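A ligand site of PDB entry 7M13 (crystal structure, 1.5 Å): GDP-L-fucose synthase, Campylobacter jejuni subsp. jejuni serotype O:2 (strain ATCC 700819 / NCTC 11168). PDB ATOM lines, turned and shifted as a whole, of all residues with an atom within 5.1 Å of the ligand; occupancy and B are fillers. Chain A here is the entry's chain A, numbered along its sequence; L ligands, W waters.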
ATOM      1  N   GLY A  15       5.048  -9.120 -25.644  1.00  0.00           N
ATOM      2  CA  GLY A  15       4.383  -9.263 -24.350  1.00  0.00           C
ATOM      3  C   GLY A  15       4.048  -7.924 -23.712  1.00  0.00           C
ATOM      4  O   GLY A  15       4.175  -7.755 -22.464  1.00  0.00           O
ATOM      5  N   HIS A  16       3.550  -6.967 -24.501  1.00  0.00           N
ATOM      6  CA  HIS A  16       3.453  -5.559 -24.041  1.00  0.00           C
ATOM      7  C   HIS A  16       2.342  -5.356 -23.008  1.00  0.00           C
ATOM      8  O   HIS A  16       2.346  -4.290 -22.378  1.00  0.00           O
ATOM      9  CB  HIS A  16       3.250  -4.652 -25.260  1.00  0.00           C
ATOM     10  CG  HIS A  16       1.902  -4.755 -25.868  1.00  0.00           C
ATOM     11  ND1 HIS A  16       1.567  -5.820 -26.681  1.00  0.00           N
ATOM     12  CD2 HIS A  16       0.819  -3.943 -25.815  1.00  0.00           C
ATOM     13  CE1 HIS A  16       0.320  -5.627 -27.108  1.00  0.00           C
ATOM     14  NE2 HIS A  16      -0.152  -4.496 -26.583  1.00  0.00           N
ATOM     15  N   LYS A  17       1.419  -6.297 -22.839  1.00  0.00           N
ATOM     16  CA  LYS A  17       0.305  -6.142 -21.855  1.00  0.00           C
ATOM     17  C   LYS A  17       0.738  -6.644 -20.481  1.00  0.00           C
ATOM     18  O   LYS A  17      -0.024  -6.425 -19.505  1.00  0.00           O
ATOM     19  CB  LYS A  17      -0.962  -6.853 -22.335  1.00  0.00           C
ATOM     20  CG  LYS A  17      -1.646  -6.196 -23.526  1.00  0.00           C
ATOM     21  CD  LYS A  17      -1.922  -4.723 -23.340  1.00  0.00           C
ATOM     22  CE  LYS A  17      -2.915  -4.414 -22.235  1.00  0.00           C
ATOM     23  NZ  LYS A  17      -4.148  -3.788 -22.767  1.00  0.00           N
ATOM     24  N   GLY A  18       1.914  -7.236 -20.352  1.00  0.00           N
ATOM     25  CA  GLY A  18       2.399  -7.793 -19.093  1.00  0.00           C
ATOM     26  C   GLY A  18       2.981  -6.727 -18.199  1.00  0.00           C
ATOM     27  O   GLY A  18       2.965  -5.525 -18.544  1.00  0.00           O
ATOM     28  N   THR A  19       3.485  -7.106 -17.043  1.00  0.00           N
ATOM     29  CA  THR A  19       3.979  -6.097 -16.086  1.00  0.00           C
ATOM     30  C   THR A  19       5.141  -5.307 -16.693  1.00  0.00           C
ATOM     31  O   THR A  19       5.147  -4.037 -16.662  1.00  0.00           O
ATOM     32  CB  THR A  19       4.363  -6.758 -14.772  1.00  0.00           C
ATOM     33  OG1 THR A  19       3.196  -7.446 -14.282  1.00  0.00           O
ATOM     34  CG2 THR A  19       4.818  -5.747 -13.744  1.00  0.00           C
ATOM     35  N   ALA A  20       6.203  -6.017 -17.100  1.00  0.00           N
ATOM     36  CA  ALA A  20       7.392  -5.361 -17.675  1.00  0.00           C
ATOM     37  C   ALA A  20       7.013  -4.674 -18.978  1.00  0.00           C
ATOM     38  O   ALA A  20       7.508  -3.544 -19.237  1.00  0.00           O
ATOM     39  CB  ALA A  20       8.469  -6.360 -17.875  1.00  0.00           C
ATOM     40  N   GLY A  21       6.232  -5.328 -19.809  1.00  0.00           N
ATOM     41  CA  GLY A  21       5.876  -4.741 -21.105  1.00  0.00           C
ATOM     42  C   GLY A  21       5.130  -3.446 -20.943  1.00  0.00           C
ATOM     43  O   GLY A  21       5.427  -2.500 -21.672  1.00  0.00           O
ATOM     44  N   THR A  40      -0.971  -8.073 -29.536  1.00  0.00           N
ATOM     45  CA  THR A  40      -1.553  -8.918 -28.492  1.00  0.00           C
ATOM     46  C   THR A  40      -1.325 -10.403 -28.819  1.00  0.00           C
ATOM     47  O   THR A  40      -0.964 -10.743 -29.970  1.00  0.00           O
ATOM     48  CB  THR A  40      -3.062  -8.675 -28.337  1.00  0.00           C
ATOM     49  OG1 THR A  40      -3.639  -9.149 -29.550  1.00  0.00           O
ATOM     50  CG2 THR A  40      -3.423  -7.223 -28.081  1.00  0.00           C
ATOM     51  N   ARG A  41      -1.527 -11.272 -27.845  1.00  0.00           N
ATOM     52  CA  ARG A  41      -1.466 -12.742 -28.058  1.00  0.00           C
ATOM     53  C   ARG A  41      -2.420 -13.150 -29.173  1.00  0.00           C
ATOM     54  O   ARG A  41      -2.087 -14.042 -29.962  1.00  0.00           O
ATOM     55  CB  ARG A  41      -1.777 -13.474 -26.763  1.00  0.00           C
ATOM     56  CG  ARG A  41      -1.729 -14.986 -26.925  1.00  0.00           C
ATOM     57  CD  ARG A  41      -2.388 -15.666 -25.739  1.00  0.00           C
ATOM     58  NE  ARG A  41      -1.706 -15.418 -24.472  1.00  0.00           N
ATOM     59  CZ  ARG A  41      -0.816 -16.228 -23.910  1.00  0.00           C
ATOM     60  NH1 ARG A  41      -0.446 -17.352 -24.505  1.00  0.00           N
ATOM     61  NH2 ARG A  41      -0.300 -15.906 -22.756  1.00  0.00           N
ATOM     62  N   GLN A  42      -3.602 -12.532 -29.249  1.00  0.00           N
ATOM     63  CA  GLN A  42      -4.644 -12.885 -30.251  1.00  0.00           C
ATOM     64  C   GLN A  42      -4.152 -12.506 -31.652  1.00  0.00           C
ATOM     65  O   GLN A  42      -4.395 -13.243 -32.627  1.00  0.00           O
ATOM     66  CB  GLN A  42      -5.948 -12.195 -29.821  1.00  0.00           C
ATOM     67  CG  GLN A  42      -6.577 -12.767 -28.552  1.00  0.00           C
ATOM     68  CD  GLN A  42      -5.876 -12.520 -27.234  1.00  0.00           C
ATOM     69  OE1 GLN A  42      -5.794 -13.424 -26.393  1.00  0.00           O
ATOM     70  NE2 GLN A  42      -5.355 -11.311 -27.012  1.00  0.00           N
ATOM     71  N   LEU A  44      -0.807 -12.204 -32.465  1.00  0.00           N
ATOM     72  CA  LEU A  44       0.489 -12.852 -32.786  1.00  0.00           C
ATOM     73  C   LEU A  44       0.806 -13.835 -31.660  1.00  0.00           C
ATOM     74  O   LEU A  44       1.163 -13.391 -30.544  1.00  0.00           O
ATOM     75  CB  LEU A  44       1.596 -11.814 -32.930  1.00  0.00           C
ATOM     76  CG  LEU A  44       3.022 -12.368 -33.121  1.00  0.00           C
ATOM     77  CD1 LEU A  44       3.117 -13.271 -34.350  1.00  0.00           C
ATOM     78  CD2 LEU A  44       4.035 -11.247 -33.199  1.00  0.00           C
ATOM     79  N   ASP A  45       0.626 -15.134 -31.925  1.00  0.00           N
ATOM     80  CA  ASP A  45       0.989 -16.182 -30.944  1.00  0.00           C
ATOM     81  C   ASP A  45       2.480 -16.470 -31.056  1.00  0.00           C
ATOM     82  O   ASP A  45       2.914 -17.018 -32.069  1.00  0.00           O
ATOM     83  CB  ASP A  45       0.214 -17.453 -31.266  1.00  0.00           C
ATOM     84  CG  ASP A  45       0.511 -18.619 -30.368  1.00  0.00           C
ATOM     85  OD1 ASP A  45       1.282 -18.470 -29.391  1.00  0.00           O
ATOM     86  OD2 ASP A  45      -0.083 -19.695 -30.658  1.00  0.00           O
ATOM     87  N   LEU A  46       3.247 -16.074 -30.040  1.00  0.00           N
ATOM     88  CA  LEU A  46       4.741 -16.127 -30.161  1.00  0.00           C
ATOM     89  C   LEU A  46       5.258 -17.574 -30.039  1.00  0.00           C
ATOM     90  O   LEU A  46       6.436 -17.771 -30.373  1.00  0.00           O
ATOM     91  CB  LEU A  46       5.358 -15.261 -29.073  1.00  0.00           C
ATOM     92  CG  LEU A  46       5.101 -13.763 -29.205  1.00  0.00           C
ATOM     93  CD1 LEU A  46       5.542 -13.010 -27.954  1.00  0.00           C
ATOM     94  CD2 LEU A  46       5.724 -13.217 -30.447  1.00  0.00           C
ATOM     95  N   VAL A  47       4.426 -18.537 -29.702  1.00  0.00           N
ATOM     96  CA  VAL A  47       4.796 -19.983 -29.805  1.00  0.00           C
ATOM     97  C   VAL A  47       4.790 -20.447 -31.273  1.00  0.00           C
ATOM     98  O   VAL A  47       5.435 -21.438 -31.589  1.00  0.00           O
ATOM     99  CB  VAL A  47       3.889 -20.803 -28.873  1.00  0.00           C
ATOM    100  CG1 VAL A  47       4.027 -22.305 -29.078  1.00  0.00           C
ATOM    101  CG2 VAL A  47       4.187 -20.448 -27.436  1.00  0.00           C
ATOM    102  N   LEU A  66      12.075  -8.390 -25.283  1.00  0.00           N
ATOM    103  CA  LEU A  66      11.387  -9.697 -25.268  1.00  0.00           C
ATOM    104  C   LEU A  66      10.886  -9.921 -23.846  1.00  0.00           C
ATOM    105  O   LEU A  66      11.639 -10.489 -23.018  1.00  0.00           O
ATOM    106  CB  LEU A  66      12.330 -10.792 -25.780  1.00  0.00           C
ATOM    107  CG  LEU A  66      11.781 -12.218 -25.742  1.00  0.00           C
ATOM    108  CD1 LEU A  66      10.375 -12.274 -26.325  1.00  0.00           C
ATOM    109  CD2 LEU A  66      12.744 -13.150 -26.438  1.00  0.00           C
ATOM    110  N   THR A  67       9.669  -9.515 -23.535  1.00  0.00           N
ATOM    111  CA  THR A  67       9.111  -9.649 -22.158  1.00  0.00           C
ATOM    112  C   THR A  67       8.139 -10.823 -22.078  1.00  0.00           C
ATOM    113  O   THR A  67       7.828 -11.250 -20.944  1.00  0.00           O
ATOM    114  CB  THR A  67       8.468  -8.372 -21.613  1.00  0.00           C
ATOM    115  OG1 THR A  67       7.113  -8.286 -22.055  1.00  0.00           O
ATOM    116  CG2 THR A  67       9.204  -7.101 -21.960  1.00  0.00           C
ATOM    117  N   ALA A  68       7.690 -11.378 -23.203  1.00  0.00           N
ATOM    118  CA  ALA A  68       6.623 -12.402 -23.187  1.00  0.00           C
ATOM    119  C   ALA A  68       7.110 -13.675 -22.509  1.00  0.00           C
ATOM    120  O   ALA A  68       8.244 -14.089 -22.744  1.00  0.00           O
ATOM    121  CB  ALA A  68       6.172 -12.702 -24.599  1.00  0.00           C
ATOM    122  N   VAL A  69       6.273 -14.276 -21.689  1.00  0.00           N
ATOM    123  CA  VAL A  69       6.643 -15.470 -20.906  1.00  0.00           C
ATOM    124  C   VAL A  69       5.372 -16.185 -20.456  1.00  0.00           C
ATOM    125  O   VAL A  69       4.347 -15.509 -20.263  1.00  0.00           O
ATOM    126  CB  VAL A  69       7.506 -15.025 -19.707  1.00  0.00           C
ATOM    127  CG1 VAL A  69       6.709 -14.275 -18.653  1.00  0.00           C
ATOM    128  CG2 VAL A  69       8.270 -16.180 -19.079  1.00  0.00           C
ATOM    129  N   LEU A  70       5.477 -17.494 -20.285  1.00  0.00           N
ATOM    130  CA  LEU A  70       4.578 -18.260 -19.393  1.00  0.00           C
ATOM    131  C   LEU A  70       5.290 -18.348 -18.054  1.00  0.00           C
ATOM    132  O   LEU A  70       6.271 -19.065 -17.894  1.00  0.00           O
ATOM    133  CB  LEU A  70       4.282 -19.632 -19.979  1.00  0.00           C
ATOM    134  CG  LEU A  70       3.558 -20.585 -19.029  1.00  0.00           C
ATOM    135  CD1 LEU A  70       2.194 -20.061 -18.638  1.00  0.00           C
ATOM    136  CD2 LEU A  70       3.439 -21.951 -19.669  1.00  0.00           C
ATOM    137  N   PRO A  71       4.845 -17.547 -17.051  1.00  0.00           N
ATOM    138  CA  PRO A  71       5.593 -17.418 -15.804  1.00  0.00           C
ATOM    139  C   PRO A  71       5.310 -18.585 -14.860  1.00  0.00           C
ATOM    140  O   PRO A  71       4.261 -19.155 -14.922  1.00  0.00           O
ATOM    141  CB  PRO A  71       4.997 -16.143 -15.199  1.00  0.00           C
ATOM    142  CG  PRO A  71       3.576 -16.145 -15.664  1.00  0.00           C
ATOM    143  CD  PRO A  71       3.623 -16.718 -17.074  1.00  0.00           C
ATOM    144  N   ILE A  90       8.876 -19.351 -27.591  1.00  0.00           N
ATOM    145  CA  ILE A  90       8.864 -17.852 -27.604  1.00  0.00           C
ATOM    146  C   ILE A  90      10.273 -17.338 -27.807  1.00  0.00           C
ATOM    147  O   ILE A  90      10.550 -16.523 -28.701  1.00  0.00           O
ATOM    148  CB  ILE A  90       8.232 -17.280 -26.354  1.00  0.00           C
ATOM    149  CG1 ILE A  90       6.746 -17.633 -26.265  1.00  0.00           C
ATOM    150  CG2 ILE A  90       8.508 -15.783 -26.257  1.00  0.00           C
ATOM    151  CD1 ILE A  90       6.091 -17.384 -24.930  1.00  0.00           C
ATOM    152  N   PHE A 108      16.508  -9.423 -23.558  1.00  0.00           N
ATOM    153  CA  PHE A 108      15.775 -10.602 -23.057  1.00  0.00           C
ATOM    154  C   PHE A 108      15.881 -10.611 -21.532  1.00  0.00           C
ATOM    155  O   PHE A 108      16.826 -10.102 -20.989  1.00  0.00           O
ATOM    156  CB  PHE A 108      16.363 -11.877 -23.657  1.00  0.00           C
ATOM    157  CG  PHE A 108      15.836 -13.163 -23.076  1.00  0.00           C
ATOM    158  CD1 PHE A 108      14.476 -13.417 -23.116  1.00  0.00           C
ATOM    159  CD2 PHE A 108      16.659 -14.047 -22.418  1.00  0.00           C
ATOM    160  CE1 PHE A 108      13.954 -14.573 -22.572  1.00  0.00           C
ATOM    161  CE2 PHE A 108      16.142 -15.228 -21.890  1.00  0.00           C
ATOM    162  CZ  PHE A 108      14.776 -15.470 -21.957  1.00  0.00           C
ATOM    163  N   PHE A 109      14.856 -11.111 -20.861  1.00  0.00           N
ATOM    164  CA  PHE A 109      14.828 -11.154 -19.369  1.00  0.00           C
ATOM    165  C   PHE A 109      14.911 -12.589 -18.858  1.00  0.00           C
ATOM    166  O   PHE A 109      14.166 -13.489 -19.364  1.00  0.00           O
ATOM    167  CB  PHE A 109      13.568 -10.478 -18.847  1.00  0.00           C
ATOM    168  CG  PHE A 109      13.496  -9.030 -19.221  1.00  0.00           C
ATOM    169  CD1 PHE A 109      14.081  -8.055 -18.448  1.00  0.00           C
ATOM    170  CD2 PHE A 109      12.969  -8.648 -20.452  1.00  0.00           C
ATOM    171  CE1 PHE A 109      14.061  -6.724 -18.825  1.00  0.00           C
ATOM    172  CE2 PHE A 109      12.939  -7.330 -20.829  1.00  0.00           C
ATOM    173  CZ  PHE A 109      13.509  -6.359 -20.022  1.00  0.00           C
ATOM    174  N   GLY A 110      15.865 -12.831 -17.970  1.00  0.00           N
ATOM    175  CA  GLY A 110      16.011 -14.074 -17.235  1.00  0.00           C
ATOM    176  C   GLY A 110      15.385 -13.975 -15.850  1.00  0.00           C
ATOM    177  O   GLY A 110      15.057 -12.863 -15.361  1.00  0.00           O
ATOM    178  N   SER A 111      15.379 -15.109 -15.164  1.00  0.00           N
ATOM    179  CA  SER A 111      14.883 -15.248 -13.783  1.00  0.00           C
ATOM    180  C   SER A 111      15.986 -15.825 -12.915  1.00  0.00           C
ATOM    181  O   SER A 111      16.703 -16.687 -13.429  1.00  0.00           O
ATOM    182  CB  SER A 111      13.682 -16.165 -13.763  1.00  0.00           C
ATOM    183  OG  SER A 111      13.379 -16.636 -12.466  1.00  0.00           O
ATOM    184  N   PHE A 140      11.334 -24.380 -15.912  1.00  0.00           N
ATOM    185  CA  PHE A 140      11.296 -22.932 -16.208  1.00  0.00           C
ATOM    186  C   PHE A 140      12.713 -22.367 -16.217  1.00  0.00           C
ATOM    187  O   PHE A 140      13.135 -21.669 -17.153  1.00  0.00           O
ATOM    188  CB  PHE A 140      10.379 -22.239 -15.208  1.00  0.00           C
ATOM    189  CG  PHE A 140      10.316 -20.750 -15.385  1.00  0.00           C
ATOM    190  CD1 PHE A 140       9.496 -20.185 -16.346  1.00  0.00           C
ATOM    191  CD2 PHE A 140      11.084 -19.929 -14.597  1.00  0.00           C
ATOM    192  CE1 PHE A 140       9.431 -18.819 -16.503  1.00  0.00           C
ATOM    193  CE2 PHE A 140      11.003 -18.551 -14.738  1.00  0.00           C
ATOM    194  CZ  PHE A 140      10.162 -18.006 -15.678  1.00  0.00           C
ATOM    195  N   LYS A 144      15.008 -20.646 -19.219  1.00  0.00           N
ATOM    196  CA  LYS A 144      15.671 -19.342 -19.120  1.00  0.00           C
ATOM    197  C   LYS A 144      17.169 -19.508 -19.402  1.00  0.00           C
ATOM    198  O   LYS A 144      17.755 -18.596 -20.021  1.00  0.00           O
ATOM    199  CB  LYS A 144      15.409 -18.728 -17.753  1.00  0.00           C
ATOM    200  CG  LYS A 144      14.010 -18.204 -17.577  1.00  0.00           C
ATOM    201  CD  LYS A 144      13.579 -17.203 -18.621  1.00  0.00           C
ATOM    202  CE  LYS A 144      12.384 -16.387 -18.149  1.00  0.00           C
ATOM    203  NZ  LYS A 144      12.028 -15.328 -19.139  1.00  0.00           N
ATOM    204  N   LEU A 167      16.592 -11.025 -13.255  1.00  0.00           N
ATOM    205  CA  LEU A 167      16.014 -10.453 -12.012  1.00  0.00           C
ATOM    206  C   LEU A 167      15.326 -11.537 -11.171  1.00  0.00           C
ATOM    207  O   LEU A 167      15.069 -12.630 -11.682  1.00  0.00           O
ATOM    208  CB  LEU A 167      15.061  -9.327 -12.371  1.00  0.00           C
ATOM    209  CG  LEU A 167      13.825  -9.726 -13.157  1.00  0.00           C
ATOM    210  CD1 LEU A 167      12.606  -8.927 -12.651  1.00  0.00           C
ATOM    211  CD2 LEU A 167      13.992  -9.543 -14.655  1.00  0.00           C
ATOM    212  N   ASN A 168      15.018 -11.211  -9.933  1.00  0.00           N
ATOM    213  CA  ASN A 168      14.327 -12.174  -9.045  1.00  0.00           C
ATOM    214  C   ASN A 168      12.835 -11.893  -8.954  1.00  0.00           C
ATOM    215  O   ASN A 168      12.077 -12.882  -9.178  1.00  0.00           O
ATOM    216  CB  ASN A 168      14.976 -12.212  -7.669  1.00  0.00           C
ATOM    217  CG  ASN A 168      16.250 -13.007  -7.751  1.00  0.00           C
ATOM    218  OD1 ASN A 168      16.279 -14.092  -8.329  1.00  0.00           O
ATOM    219  ND2 ASN A 168      17.272 -12.471  -7.115  1.00  0.00           N
ATOM    220  N   ASN A 169      12.425 -10.700  -8.554  1.00  0.00           N
ATOM    221  CA  ASN A 169      10.986 -10.440  -8.260  1.00  0.00           C
ATOM    222  C   ASN A 169      10.637  -9.029  -8.672  1.00  0.00           C
ATOM    223  O   ASN A 169      11.281  -8.077  -8.193  1.00  0.00           O
ATOM    224  CB  ASN A 169      10.625 -10.571  -6.787  1.00  0.00           C
ATOM    225  CG  ASN A 169      10.796 -11.958  -6.261  1.00  0.00           C
ATOM    226  OD1 ASN A 169      10.111 -12.885  -6.727  1.00  0.00           O
ATOM    227  ND2 ASN A 169      11.701 -12.101  -5.328  1.00  0.00           N
ATOM    228  N   LEU A 170       9.641  -8.895  -9.525  1.00  0.00           N
ATOM    229  CA  LEU A 170       9.155  -7.617 -10.082  1.00  0.00           C
ATOM    230  C   LEU A 170       7.903  -7.194  -9.339  1.00  0.00           C
ATOM    231  O   LEU A 170       7.051  -8.074  -9.065  1.00  0.00           O
ATOM    232  CB  LEU A 170       8.886  -7.892 -11.559  1.00  0.00           C
ATOM    233  CG  LEU A 170       8.516  -6.712 -12.422  1.00  0.00           C
ATOM    234  CD1 LEU A 170       9.606  -5.654 -12.455  1.00  0.00           C
ATOM    235  CD2 LEU A 170       8.211  -7.187 -13.825  1.00  0.00           C
ATOM    236  N   ARG A 183       0.442 -11.181  -4.841  1.00  0.00           N
ATOM    237  CA  ARG A 183       1.868 -11.435  -4.512  1.00  0.00           C
ATOM    238  C   ARG A 183       2.171 -10.883  -3.105  1.00  0.00           C
ATOM    239  O   ARG A 183       1.288 -10.267  -2.486  1.00  0.00           O
ATOM    240  CB  ARG A 183       2.713 -10.816  -5.629  1.00  0.00           C
ATOM    241  CG  ARG A 183       2.305 -11.283  -7.027  1.00  0.00           C
ATOM    242  CD  ARG A 183       2.875 -10.399  -8.106  1.00  0.00           C
ATOM    243  NE  ARG A 183       4.259 -10.754  -8.386  1.00  0.00           N
ATOM    244  CZ  ARG A 183       4.645 -11.590  -9.353  1.00  0.00           C
ATOM    245  NH1 ARG A 183       3.762 -12.125 -10.167  1.00  0.00           N
ATOM    246  NH2 ARG A 183       5.934 -11.855  -9.509  1.00  0.00           N
ATOM    247  N   LEU A 250      12.960  -1.584 -13.645  1.00  0.00           N
ATOM    248  CA  LEU A 250      13.195  -2.595 -14.707  1.00  0.00           C
ATOM    249  C   LEU A 250      13.179  -1.888 -16.065  1.00  0.00           C
ATOM    250  O   LEU A 250      14.087  -2.122 -16.895  1.00  0.00           O
ATOM    251  CB  LEU A 250      12.145  -3.706 -14.673  1.00  0.00           C
ATOM    252  CG  LEU A 250      12.252  -4.746 -15.798  1.00  0.00           C
ATOM    253  CD1 LEU A 250      11.741  -6.103 -15.355  1.00  0.00           C
ATOM    254  CD2 LEU A 250      11.485  -4.318 -17.036  1.00  0.00           C
HETATM  255  P1  LIG L   1       3.792 -11.123 -17.376  1.00  0.00           P
HETATM  256  O1  LIG L   1       3.376 -12.511 -16.973  1.00  0.00           O
HETATM  257  O2  LIG L   1       3.236  -9.978 -16.599  1.00  0.00           O
HETATM  258  O3  LIG L   1       3.454 -10.845 -18.889  1.00  0.00           O
HETATM  259  C1  LIG L   1       3.715 -11.840 -19.887  1.00  0.00           C
HETATM  260  C2  LIG L   1       3.102 -11.357 -21.175  1.00  0.00           C
HETATM  261  O4  LIG L   1       3.499 -12.260 -22.229  1.00  0.00           O
HETATM  262  C3  LIG L   1       1.568 -11.368 -21.126  1.00  0.00           C
HETATM  263  O5  LIG L   1       1.046 -10.136 -21.593  1.00  0.00           O
HETATM  264  C4  LIG L   1       1.211 -12.525 -22.046  1.00  0.00           C
HETATM  265  O6  LIG L   1       0.031 -12.273 -22.823  1.00  0.00           O
HETATM  266  C5  LIG L   1       2.377 -12.499 -23.041  1.00  0.00           C
HETATM  267  N1  LIG L   1       2.552 -13.768 -23.706  1.00  0.00           N
HETATM  268  C6  LIG L   1       2.811 -14.989 -23.131  1.00  0.00           C
HETATM  269  N2  LIG L   1       2.759 -15.993 -23.972  1.00  0.00           N
HETATM  270  C7  LIG L   1       2.502 -15.390 -25.196  1.00  0.00           C
HETATM  271  C8  LIG L   1       2.356 -15.913 -26.495  1.00  0.00           C
HETATM  272  N3  LIG L   1       2.376 -17.217 -26.798  1.00  0.00           N
HETATM  273  N4  LIG L   1       2.085 -15.042 -27.498  1.00  0.00           N
HETATM  274  C9  LIG L   1       1.986 -13.735 -27.190  1.00  0.00           C
HETATM  275  N5  LIG L   1       2.114 -13.136 -26.013  1.00  0.00           N
HETATM  276  C10 LIG L   1       2.353 -14.026 -25.045  1.00  0.00           C
HETATM  277  O7  LIG L   1       5.410 -11.083 -17.436  1.00  0.00           O
HETATM  278  P2  LIG L   1       6.329 -10.126 -16.573  1.00  0.00           P
HETATM  279  O8  LIG L   1       6.093 -10.378 -15.140  1.00  0.00           O
HETATM  280  O9  LIG L   1       6.185  -8.782 -17.157  1.00  0.00           O
HETATM  281  O10 LIG L   1       7.776 -10.709 -16.947  1.00  0.00           O
HETATM  282  C11 LIG L   1       8.584 -10.091 -17.931  1.00  0.00           C
HETATM  283  C12 LIG L   1       9.862 -10.867 -18.024  1.00  0.00           C
HETATM  284  O11 LIG L   1      10.559 -10.757 -16.766  1.00  0.00           O
HETATM  285  C13 LIG L   1       9.705 -12.376 -18.294  1.00  0.00           C
HETATM  286  O12 LIG L   1      10.784 -12.823 -19.114  1.00  0.00           O
HETATM  287  C14 LIG L   1       9.792 -12.947 -16.901  1.00  0.00           C
HETATM  288  O13 LIG L   1      10.152 -14.327 -16.819  1.00  0.00           O
HETATM  289  C15 LIG L   1      10.836 -12.051 -16.267  1.00  0.00           C
HETATM  290  N6  LIG L   1      10.785 -12.060 -14.790  1.00  0.00           N
HETATM  291  C16 LIG L   1       9.691 -11.601 -14.091  1.00  0.00           C
HETATM  292  C17 LIG L   1       9.596 -11.714 -12.739  1.00  0.00           C
HETATM  293  C18 LIG L   1       8.416 -11.244 -12.008  1.00  0.00           C
HETATM  294  O14 LIG L   1       8.464 -11.250 -10.774  1.00  0.00           O
HETATM  295  N7  LIG L   1       7.336 -10.815 -12.675  1.00  0.00           N
HETATM  296  C19 LIG L   1      10.737 -12.305 -11.985  1.00  0.00           C
HETATM  297  C20 LIG L   1      11.845 -12.753 -12.796  1.00  0.00           C
HETATM  298  C21 LIG L   1      11.824 -12.658 -14.111  1.00  0.00           C
HETATM  299  P3  LIG L   1      -1.448 -12.496 -22.179  1.00  0.00           P
HETATM  300  O15 LIG L   1      -1.577 -11.244 -21.360  1.00  0.00           O
HETATM  301  O16 LIG L   1      -1.535 -13.782 -21.428  1.00  0.00           O
HETATM  302  O17 LIG L   1      -2.316 -12.476 -23.436  1.00  0.00           O
HETATM  303  O   HOH W   1      -0.867 -12.390 -18.322  1.00  0.00           O
HETATM  304  O   HOH W   2      -3.831  -9.448 -21.775  1.00  0.00           O
HETATM  305  O   HOH W   3      -1.898 -10.204 -25.126  1.00  0.00           O
HETATM  306  O   HOH W   4       2.605 -19.037 -24.443  1.00  0.00           O
HETATM  307  O   HOH W   5       4.003 -10.071 -13.820  1.00  0.00           O
HETATM  308  O   HOH W   6       6.262 -13.127 -14.705  1.00  0.00           O
HETATM  309  O   HOH W   7       1.239 -13.913 -17.636  1.00  0.00           O
HETATM  310  O   HOH W   8      10.713 -13.023 -21.835  1.00  0.00           O
HETATM  311  O   HOH W   9      -4.830 -12.784 -23.734  1.00  0.00           O
HETATM  312  O   HOH W  10       5.487  -8.064 -19.675  1.00  0.00           O
HETATM  313  O   HOH W  11       0.687  -9.400 -15.980  1.00  0.00           O
HETATM  314  O   HOH W  12       1.928 -10.145 -26.350  1.00  0.00           O
HETATM  315  O   HOH W  13       8.297 -15.111 -14.932  1.00  0.00           O
HETATM  316  O   HOH W  14       0.691  -8.894 -24.222  1.00  0.00           O
HETATM  317  O   HOH W  15       3.133 -12.642 -14.306  1.00  0.00           O
HETATM  318  O   HOH W  16       8.445 -13.267  -8.856  1.00  0.00           O
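The backbone NH (N) of Ala 20 is in hydrogen-bond range of an oxygen (O9) of the ligand. The guanidinium group (NH2) of Arg 41 lies within salt-bridge range of an oxygen (O16) of the ligand (2.8 Å). An oxygen (O12) of the ligand sits at hydrogen-bond distance from the side-chain amino group (NZ) of Lys 144, 2.8 Å away. NH2 of Arg 183 is in hydrogen-bond range of O14 of the ligand (2.9 Å). The backbone NH of Leu 170 is in hydrogen-bond range of an oxygen (O14) of the ligand (2.9 Å). O2 of the ligand is in hydrogen-bond range of N of Thr 19. O2 of the ligand lies within hydrogen-bond range of OG1 of Thr 19 (3.4 Å). N4 of the ligand is in hydrogen-bond range of N of Leu 46, 3.0 Å away. The side-chain carboxylate (OD1) of Asp 45 is in hydrogen-bond range of a nitrogen (N3) of the ligand, 3.1 Å away. O5 of the ligand is in hydrogen-bond range of N of Gly 18, at 3.3 Å. The backbone NH (N) of Val 69 sits at hydrogen-bond distance from an oxygen (O4) of the ligand, 3.5 Å away. O12 of the ligand sits at hydrogen-bond distance from O of Phe 109, at 3.5 Å.
NZ of Lys 144 sits at hydrogen-bond distance from O of Phe 109 (2.8 Å). The backbone NH (N) of Val 47 sits close to the side-chain carboxylate (OD1) of Asp 45 (3.2 Å). The side-chain hydroxyl of Thr 67 sits at hydrogen-bond distance from the backbone carbonyl oxygen of Gly 15. The backbone carbonyl oxygen of Gly 110 is in hydrogen-bond range of the backbone NH of Leu 167.
Gly 15 touches the ligand. C of Lys 17 touches O5 of the ligand, at 3.7 Å. Leu 44 touches the ligand (O to C9, 3.5 Å). Val 47 touches the ligand. O of Thr 67 touches C11 of the ligand, at 3.3 Å. CA of Ala 68 touches O4 of the ligand, 3.3 Å away. Pro 71 touches the ligand (CG to O1, 3.9 Å). Ile 90 touches the ligand (CD1 to N2, 3.7 Å). Gly 110 touches the ligand (O to C21, 3.5 Å). Ser 111 touches the ligand (CB to C21, 3.98 Å). CZ of Phe 140 touches O13 of the ligand, 3.9 Å away. Leu 167 touches the ligand (O to C20, 3.4 Å). Asn 168 touches the ligand. Asn 169 touches the ligand. Hydrophobic or aromatic side chains within 4 Å of the ligand: Ala 20, Leu 46, Val 47, Ala 68, Val 69, Pro 71, Ile 90, Phe 109, Phe 140, Leu 167 and Leu 170.
Water W9 bridges an oxygen (O17) of the ligand (2.6 Å) and the side-chain amide oxygen (OE1) of Gln 42 (2.9 Å). Water W16 lies within hydrogen-bond range of OD1 of Asn 169 (2.7 Å), O14 of the ligand (2.8 Å) and NH2 of Arg 183 (3.0 Å). Water W3 lies within hydrogen-bond range of an oxygen (O17) of the ligand (2.9 Å) and the backbone NH (N) of Arg 41 (2.9 Å). Water W14 lies within hydrogen-bond range of O5 of the ligand (2.9 Å), N of Lys 17 (3.0 Å) and N of His 16 (3.5 Å). Water W4 bridges N3 of the ligand (3.0 Å) and NH1 of Arg 41 (3.5 Å). Water W12 lies within hydrogen-bond range of a nitrogen (N5) of the ligand and the backbone NH (N) of Gly 15.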
